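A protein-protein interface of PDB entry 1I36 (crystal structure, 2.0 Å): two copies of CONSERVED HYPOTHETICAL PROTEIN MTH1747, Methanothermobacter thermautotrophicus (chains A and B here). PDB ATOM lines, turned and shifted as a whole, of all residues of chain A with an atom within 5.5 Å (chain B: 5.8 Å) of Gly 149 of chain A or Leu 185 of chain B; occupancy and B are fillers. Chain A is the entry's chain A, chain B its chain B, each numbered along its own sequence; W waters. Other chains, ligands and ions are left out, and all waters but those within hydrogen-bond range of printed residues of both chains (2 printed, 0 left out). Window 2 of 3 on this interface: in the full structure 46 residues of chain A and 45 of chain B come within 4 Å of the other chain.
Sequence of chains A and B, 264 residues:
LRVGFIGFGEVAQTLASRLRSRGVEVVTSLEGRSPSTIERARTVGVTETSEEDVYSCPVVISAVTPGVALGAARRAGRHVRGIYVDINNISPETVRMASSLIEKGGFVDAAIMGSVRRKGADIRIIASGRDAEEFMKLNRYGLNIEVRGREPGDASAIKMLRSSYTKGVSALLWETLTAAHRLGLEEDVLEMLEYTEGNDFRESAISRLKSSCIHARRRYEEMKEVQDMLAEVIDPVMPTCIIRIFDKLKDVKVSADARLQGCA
The guanidinium group (NH1) of Arg 148 of chain A is in salt-bridge range of the side-chain carboxylate (OD1) of Asp 188 of chain B (3.0 Å). The backbone NH of Gly 149 of chain A is in hydrogen-bond range of the side-chain carboxylate of Asp 188 of chain B.
O of Ala 127 of chain A sits at hydrogen-bond distance from N of Arg 148 of chain A (2.9 Å). N of Asp 154 of chain A is in hydrogen-bond range of OG of Ser 128 of chain A, 3.5 Å away. The backbone NH (N) of Arg 150 of chain A lies within hydrogen-bond range of the side-chain carboxylate (OD2) of Asp 154 of chain A (2.7 Å). N of Glu 151 of chain A lies within hydrogen-bond range of OD2 of Asp 154 of chain A, 3.0 Å away. O of Ala 180 of chain B is in hydrogen-bond range of N of Leu 185 of chain B (2.8 Å).
Among the printed residues, merely in contact across the chains: Ala 157 of chain A with Leu 183 of chain B (3.5 Å), Asp 154 of chain A with Leu 185 of chain B (3.8 Å), Leu 161 of chain A with Ala 180 of chain B (3.8 Å), Gly 149 of chain A with Leu 185 of chain B (3.8 Å), Leu 161 of chain A with Val 189 of chain B (3.9 Å), Ile 158 of chain A with Asp 188 of chain B (3.9 Å) and Ala 157 of chain A with Leu 185 of chain B (3.98 Å).
Of chain B, only Leu 185 (3.8 Å) and Asp 188 (3.2 Å) come within 4 Å of Gly 149 of chain A. Printed residues of chain B within 4 Å of Asp 154 of chain A: Leu 185. Printed residues of chain B within 4 Å of Leu 161 of chain A: Ala 180 (3.8 Å) and Val 189 (3.9 Å). Of the printed residues of chain A, Asp 188 of chain B touches Arg 148 (3.0 Å), Gly 149 (3.2 Å) and Ile 158 (3.9 Å). Leu 190 of chain B touches none of the printed residues of chain A. The nearest printed residue of chain B that does not touch Arg 148 of chain A is Glu 187 of chain B (5.0 Å).
Along chain B the printed residues that touch a printed residue of chain A span positions 180 to 189.
No position is printed for both chains.
Water W1 lies within hydrogen-bond range of OD1 of Asp 154 of chain A and O of Leu 183 of chain B. Water W2 lies within hydrogen-bond range of the backbone carbonyl oxygen of Leu 183 of chain B, the side-chain carboxylate of Asp 154 of chain A and the guanidinium group of Arg 150 of chain A.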
ATOM      1  N   ALA A 127     -30.230  -0.352 -20.433  1.00  0.00           N
ATOM      2  CA  ALA A 127     -30.630  -1.665 -20.957  1.00  0.00           C
ATOM      3  C   ALA A 127     -29.936  -2.788 -20.205  1.00  0.00           C
ATOM      4  O   ALA A 127     -28.749  -2.693 -19.850  1.00  0.00           O
ATOM      5  CB  ALA A 127     -30.285  -1.731 -22.480  1.00  0.00           C
ATOM      6  N   SER A 128     -30.687  -3.867 -19.974  1.00  0.00           N
ATOM      7  CA  SER A 128     -30.153  -4.998 -19.236  1.00  0.00           C
ATOM      8  C   SER A 128     -30.438  -6.306 -19.966  1.00  0.00           C
ATOM      9  O   SER A 128     -31.401  -6.402 -20.725  1.00  0.00           O
ATOM     10  CB  SER A 128     -30.715  -5.007 -17.810  1.00  0.00           C
ATOM     11  OG  SER A 128     -32.086  -5.397 -17.776  1.00  0.00           O
ATOM     12  N   GLY A 129     -29.595  -7.309 -19.712  1.00  0.00           N
ATOM     13  CA  GLY A 129     -29.735  -8.604 -20.370  1.00  0.00           C
ATOM     14  C   GLY A 129     -28.406  -8.933 -21.030  1.00  0.00           C
ATOM     15  O   GLY A 129     -27.582  -8.034 -21.284  1.00  0.00           O
ATOM     16  N   VAL A 147     -25.600   0.242 -20.666  1.00  0.00           N
ATOM     17  CA  VAL A 147     -25.921  -1.078 -20.111  1.00  0.00           C
ATOM     18  C   VAL A 147     -25.880  -1.036 -18.582  1.00  0.00           C
ATOM     19  O   VAL A 147     -24.971  -0.470 -18.013  1.00  0.00           O
ATOM     20  CB  VAL A 147     -24.900  -2.166 -20.586  1.00  0.00           C
ATOM     21  CG1 VAL A 147     -25.189  -3.559 -19.883  1.00  0.00           C
ATOM     22  CG2 VAL A 147     -24.965  -2.310 -22.094  1.00  0.00           C
ATOM     23  N   ARG A 148     -26.877  -1.608 -17.922  1.00  0.00           N
ATOM     24  CA  ARG A 148     -26.899  -1.665 -16.453  1.00  0.00           C
ATOM     25  C   ARG A 148     -27.390  -3.054 -16.068  1.00  0.00           C
ATOM     26  O   ARG A 148     -28.029  -3.720 -16.881  1.00  0.00           O
ATOM     27  CB  ARG A 148     -27.887  -0.624 -15.881  1.00  0.00           C
ATOM     28  CG  ARG A 148     -27.473   0.825 -16.084  1.00  0.00           C
ATOM     29  CD  ARG A 148     -26.407   1.199 -15.084  1.00  0.00           C
ATOM     30  NE  ARG A 148     -25.884   2.555 -15.264  1.00  0.00           N
ATOM     31  CZ  ARG A 148     -25.115   3.164 -14.369  1.00  0.00           C
ATOM     32  NH1 ARG A 148     -24.790   2.536 -13.243  1.00  0.00           N
ATOM     33  NH2 ARG A 148     -24.637   4.379 -14.614  1.00  0.00           N
ATOM     34  N   GLY A 149     -27.153  -3.465 -14.824  1.00  0.00           N
ATOM     35  CA  GLY A 149     -27.629  -4.759 -14.377  1.00  0.00           C
ATOM     36  C   GLY A 149     -27.042  -5.929 -15.151  1.00  0.00           C
ATOM     37  O   GLY A 149     -25.966  -5.804 -15.750  1.00  0.00           O
ATOM     38  N   ARG A 150     -27.738  -7.065 -15.153  1.00  0.00           N
ATOM     39  CA  ARG A 150     -27.244  -8.251 -15.856  1.00  0.00           C
ATOM     40  C   ARG A 150     -28.319  -8.995 -16.653  1.00  0.00           C
ATOM     41  O   ARG A 150     -28.028  -9.594 -17.668  1.00  0.00           O
ATOM     42  CB  ARG A 150     -26.674  -9.254 -14.846  1.00  0.00           C
ATOM     43  CG  ARG A 150     -25.517  -8.747 -14.010  1.00  0.00           C
ATOM     44  CD  ARG A 150     -25.039  -9.826 -13.038  1.00  0.00           C
ATOM     45  NE  ARG A 150     -26.083 -10.250 -12.098  1.00  0.00           N
ATOM     46  CZ  ARG A 150     -25.932 -11.224 -11.199  1.00  0.00           C
ATOM     47  NH1 ARG A 150     -24.776 -11.885 -11.110  1.00  0.00           N
ATOM     48  NH2 ARG A 150     -26.938 -11.547 -10.390  1.00  0.00           N
ATOM     49  N   GLU A 151     -29.567  -8.934 -16.201  1.00  0.00           N
ATOM     50  CA  GLU A 151     -30.616  -9.701 -16.864  1.00  0.00           C
ATOM     51  C   GLU A 151     -31.895  -8.928 -17.086  1.00  0.00           C
ATOM     52  O   GLU A 151     -32.029  -7.818 -16.597  1.00  0.00           O
ATOM     53  CB  GLU A 151     -30.872 -10.974 -16.029  1.00  0.00           C
ATOM     54  CG  GLU A 151     -31.051 -10.729 -14.546  1.00  0.00           C
ATOM     55  CD  GLU A 151     -31.209 -12.025 -13.734  1.00  0.00           C
ATOM     56  OE1 GLU A 151     -30.316 -12.901 -13.767  1.00  0.00           O
ATOM     57  OE2 GLU A 151     -32.240 -12.170 -13.058  1.00  0.00           O
ATOM     58  N   GLY A 153     -35.305  -7.272 -16.695  1.00  0.00           N
ATOM     59  CA  GLY A 153     -35.937  -6.914 -15.445  1.00  0.00           C
ATOM     60  C   GLY A 153     -35.076  -5.920 -14.650  1.00  0.00           C
ATOM     61  O   GLY A 153     -35.635  -5.069 -13.940  1.00  0.00           O
ATOM     62  N   ASP A 154     -33.742  -5.979 -14.791  1.00  0.00           N
ATOM     63  CA  ASP A 154     -32.869  -5.070 -14.041  1.00  0.00           C
ATOM     64  C   ASP A 154     -33.031  -3.615 -14.427  1.00  0.00           C
ATOM     65  O   ASP A 154     -33.199  -2.773 -13.543  1.00  0.00           O
ATOM     66  CB  ASP A 154     -31.390  -5.471 -14.110  1.00  0.00           C
ATOM     67  CG  ASP A 154     -31.115  -6.801 -13.436  1.00  0.00           C
ATOM     68  OD1 ASP A 154     -31.944  -7.270 -12.629  1.00  0.00           O
ATOM     69  OD2 ASP A 154     -30.040  -7.366 -13.688  1.00  0.00           O
ATOM     70  N   ALA A 157     -36.321  -2.370 -13.189  1.00  0.00           N
ATOM     71  CA  ALA A 157     -36.256  -2.241 -11.734  1.00  0.00           C
ATOM     72  C   ALA A 157     -35.525  -0.966 -11.350  1.00  0.00           C
ATOM     73  O   ALA A 157     -35.901  -0.340 -10.388  1.00  0.00           O
ATOM     74  CB  ALA A 157     -35.529  -3.450 -11.079  1.00  0.00           C
ATOM     75  N   ILE A 158     -34.367  -0.724 -11.959  1.00  0.00           N
ATOM     76  CA  ILE A 158     -33.607   0.486 -11.686  1.00  0.00           C
ATOM     77  C   ILE A 158     -34.442   1.753 -11.951  1.00  0.00           C
ATOM     78  O   ILE A 158     -34.414   2.732 -11.171  1.00  0.00           O
ATOM     79  CB  ILE A 158     -32.327   0.546 -12.555  1.00  0.00           C
ATOM     80  CG1 ILE A 158     -31.324  -0.499 -12.080  1.00  0.00           C
ATOM     81  CG2 ILE A 158     -31.669   1.962 -12.444  1.00  0.00           C
ATOM     82  CD1 ILE A 158     -30.356  -0.988 -13.213  1.00  0.00           C
ATOM     83  N   LEU A 161     -37.108   2.057  -9.249  1.00  0.00           N
ATOM     84  CA  LEU A 161     -36.507   2.407  -7.956  1.00  0.00           C
ATOM     85  C   LEU A 161     -36.128   3.878  -7.885  1.00  0.00           C
ATOM     86  O   LEU A 161     -36.355   4.532  -6.853  1.00  0.00           O
ATOM     87  CB  LEU A 161     -35.317   1.505  -7.655  1.00  0.00           C
ATOM     88  CG  LEU A 161     -35.801   0.086  -7.329  1.00  0.00           C
ATOM     89  CD1 LEU A 161     -34.643  -0.894  -7.318  1.00  0.00           C
ATOM     90  CD2 LEU A 161     -36.513   0.083  -5.979  1.00  0.00           C
ATOM     91  N   ALA B 180     -33.317  -2.688  -4.047  1.00  0.00           N
ATOM     92  CA  ALA B 180     -32.260  -2.726  -5.044  1.00  0.00           C
ATOM     93  C   ALA B 180     -31.292  -3.852  -4.691  1.00  0.00           C
ATOM     94  O   ALA B 180     -30.838  -4.582  -5.577  1.00  0.00           O
ATOM     95  CB  ALA B 180     -31.517  -1.407  -5.069  1.00  0.00           C
ATOM     96  N   HIS B 181     -31.016  -4.015  -3.394  1.00  0.00           N
ATOM     97  CA  HIS B 181     -30.077  -5.048  -2.923  1.00  0.00           C
ATOM     98  C   HIS B 181     -30.580  -6.474  -3.221  1.00  0.00           C
ATOM     99  O   HIS B 181     -29.803  -7.336  -3.623  1.00  0.00           O
ATOM    100  CB  HIS B 181     -29.765  -4.877  -1.437  1.00  0.00           C
ATOM    101  CG  HIS B 181     -28.694  -5.800  -0.937  1.00  0.00           C
ATOM    102  ND1 HIS B 181     -28.965  -6.891  -0.138  1.00  0.00           N
ATOM    103  CD2 HIS B 181     -27.354  -5.814  -1.149  1.00  0.00           C
ATOM    104  CE1 HIS B 181     -27.839  -7.535   0.122  1.00  0.00           C
ATOM    105  NE2 HIS B 181     -26.848  -6.903  -0.480  1.00  0.00           N
ATOM    106  N   ARG B 182     -31.871  -6.726  -3.036  1.00  0.00           N
ATOM    107  CA  ARG B 182     -32.412  -8.040  -3.360  1.00  0.00           C
ATOM    108  C   ARG B 182     -32.180  -8.451  -4.811  1.00  0.00           C
ATOM    109  O   ARG B 182     -32.083  -9.637  -5.107  1.00  0.00           O
ATOM    110  CB  ARG B 182     -33.884  -8.133  -2.989  1.00  0.00           C
ATOM    111  CG  ARG B 182     -34.009  -8.355  -1.513  1.00  0.00           C
ATOM    112  CD  ARG B 182     -35.401  -8.428  -1.051  1.00  0.00           C
ATOM    113  NE  ARG B 182     -35.458  -8.421   0.409  1.00  0.00           N
ATOM    114  CZ  ARG B 182     -36.572  -8.631   1.104  1.00  0.00           C
ATOM    115  NH1 ARG B 182     -37.717  -8.872   0.470  1.00  0.00           N
ATOM    116  NH2 ARG B 182     -36.552  -8.566   2.432  1.00  0.00           N
ATOM    117  N   LEU B 183     -31.986  -7.469  -5.691  1.00  0.00           N
ATOM    118  CA  LEU B 183     -31.738  -7.719  -7.104  1.00  0.00           C
ATOM    119  C   LEU B 183     -30.269  -7.528  -7.465  1.00  0.00           C
ATOM    120  O   LEU B 183     -29.903  -7.642  -8.634  1.00  0.00           O
ATOM    121  CB  LEU B 183     -32.582  -6.758  -7.964  1.00  0.00           C
ATOM    122  CG  LEU B 183     -34.101  -6.813  -7.756  1.00  0.00           C
ATOM    123  CD1 LEU B 183     -34.818  -5.749  -8.603  1.00  0.00           C
ATOM    124  CD2 LEU B 183     -34.597  -8.203  -8.093  1.00  0.00           C
ATOM    125  N   GLY B 184     -29.448  -7.164  -6.478  1.00  0.00           N
ATOM    126  CA  GLY B 184     -28.036  -6.888  -6.726  1.00  0.00           C
ATOM    127  C   GLY B 184     -27.803  -5.588  -7.479  1.00  0.00           C
ATOM    128  O   GLY B 184     -26.761  -5.410  -8.114  1.00  0.00           O
ATOM    129  N   LEU B 185     -28.725  -4.624  -7.365  1.00  0.00           N
ATOM    130  CA  LEU B 185     -28.600  -3.378  -8.139  1.00  0.00           C
ATOM    131  C   LEU B 185     -28.360  -2.102  -7.326  1.00  0.00           C
ATOM    132  O   LEU B 185     -28.539  -0.995  -7.841  1.00  0.00           O
ATOM    133  CB  LEU B 185     -29.896  -3.185  -8.950  1.00  0.00           C
ATOM    134  CG  LEU B 185     -30.277  -4.380  -9.865  1.00  0.00           C
ATOM    135  CD1 LEU B 185     -31.682  -4.240 -10.430  1.00  0.00           C
ATOM    136  CD2 LEU B 185     -29.278  -4.428 -10.999  1.00  0.00           C
ATOM    137  N   GLU B 186     -27.990  -2.239  -6.058  1.00  0.00           N
ATOM    138  CA  GLU B 186     -27.804  -1.048  -5.218  1.00  0.00           C
ATOM    139  C   GLU B 186     -26.841  -0.004  -5.795  1.00  0.00           C
ATOM    140  O   GLU B 186     -27.119   1.200  -5.742  1.00  0.00           O
ATOM    141  CB  GLU B 186     -27.390  -1.451  -3.790  1.00  0.00           C
ATOM    142  CG  GLU B 186     -26.094  -2.234  -3.706  1.00  0.00           C
ATOM    143  CD  GLU B 186     -26.264  -3.744  -3.832  1.00  0.00           C
ATOM    144  OE1 GLU B 186     -27.174  -4.223  -4.542  1.00  0.00           O
ATOM    145  OE2 GLU B 186     -25.451  -4.461  -3.219  1.00  0.00           O
ATOM    146  N   GLU B 187     -25.727  -0.442  -6.370  1.00  0.00           N
ATOM    147  CA  GLU B 187     -24.778   0.512  -6.938  1.00  0.00           C
ATOM    148  C   GLU B 187     -25.345   1.242  -8.141  1.00  0.00           C
ATOM    149  O   GLU B 187     -25.204   2.458  -8.249  1.00  0.00           O
ATOM    150  CB  GLU B 187     -23.456  -0.170  -7.277  1.00  0.00           C
ATOM    151  CG  GLU B 187     -22.610  -0.450  -6.036  1.00  0.00           C
ATOM    152  CD  GLU B 187     -22.231   0.820  -5.281  1.00  0.00           C
ATOM    153  OE1 GLU B 187     -21.939   1.851  -5.928  1.00  0.00           O
ATOM    154  OE2 GLU B 187     -22.240   0.786  -4.040  1.00  0.00           O
ATOM    155  N   ASP B 188     -26.010   0.514  -9.037  1.00  0.00           N
ATOM    156  CA  ASP B 188     -26.623   1.162 -10.192  1.00  0.00           C
ATOM    157  C   ASP B 188     -27.671   2.163  -9.740  1.00  0.00           C
ATOM    158  O   ASP B 188     -27.769   3.261 -10.303  1.00  0.00           O
ATOM    159  CB  ASP B 188     -27.310   0.137 -11.092  1.00  0.00           C
ATOM    160  CG  ASP B 188     -26.332  -0.739 -11.825  1.00  0.00           C
ATOM    161  OD1 ASP B 188     -25.247  -0.252 -12.198  1.00  0.00           O
ATOM    162  OD2 ASP B 188     -26.668  -1.906 -12.061  1.00  0.00           O
ATOM    163  N   VAL B 189     -28.497   1.781  -8.760  1.00  0.00           N
ATOM    164  CA  VAL B 189     -29.525   2.723  -8.297  1.00  0.00           C
ATOM    165  C   VAL B 189     -28.838   3.977  -7.736  1.00  0.00           C
ATOM    166  O   VAL B 189     -29.202   5.093  -8.100  1.00  0.00           O
ATOM    167  CB  VAL B 189     -30.506   2.095  -7.263  1.00  0.00           C
ATOM    168  CG1 VAL B 189     -31.393   3.173  -6.659  1.00  0.00           C
ATOM    169  CG2 VAL B 189     -31.385   1.079  -7.961  1.00  0.00           C
ATOM    170  N   LEU B 190     -27.806   3.782  -6.912  1.00  0.00           N
ATOM    171  CA  LEU B 190     -27.063   4.920  -6.351  1.00  0.00           C
ATOM    172  C   LEU B 190     -26.490   5.805  -7.455  1.00  0.00           C
ATOM    173  O   LEU B 190     -26.586   7.026  -7.385  1.00  0.00           O
ATOM    174  CB  LEU B 190     -25.957   4.444  -5.425  1.00  0.00           C
ATOM    175  CG  LEU B 190     -26.433   4.077  -4.031  1.00  0.00           C
ATOM    176  CD1 LEU B 190     -25.350   3.319  -3.330  1.00  0.00           C
ATOM    177  CD2 LEU B 190     -26.822   5.352  -3.268  1.00  0.00           C
HETATM  178  O   HOH W   1     -31.668  -9.172 -10.555  1.00  0.00           O
HETATM  179  O   HOH W   2     -28.473  -8.344 -11.231  1.00  0.00           O
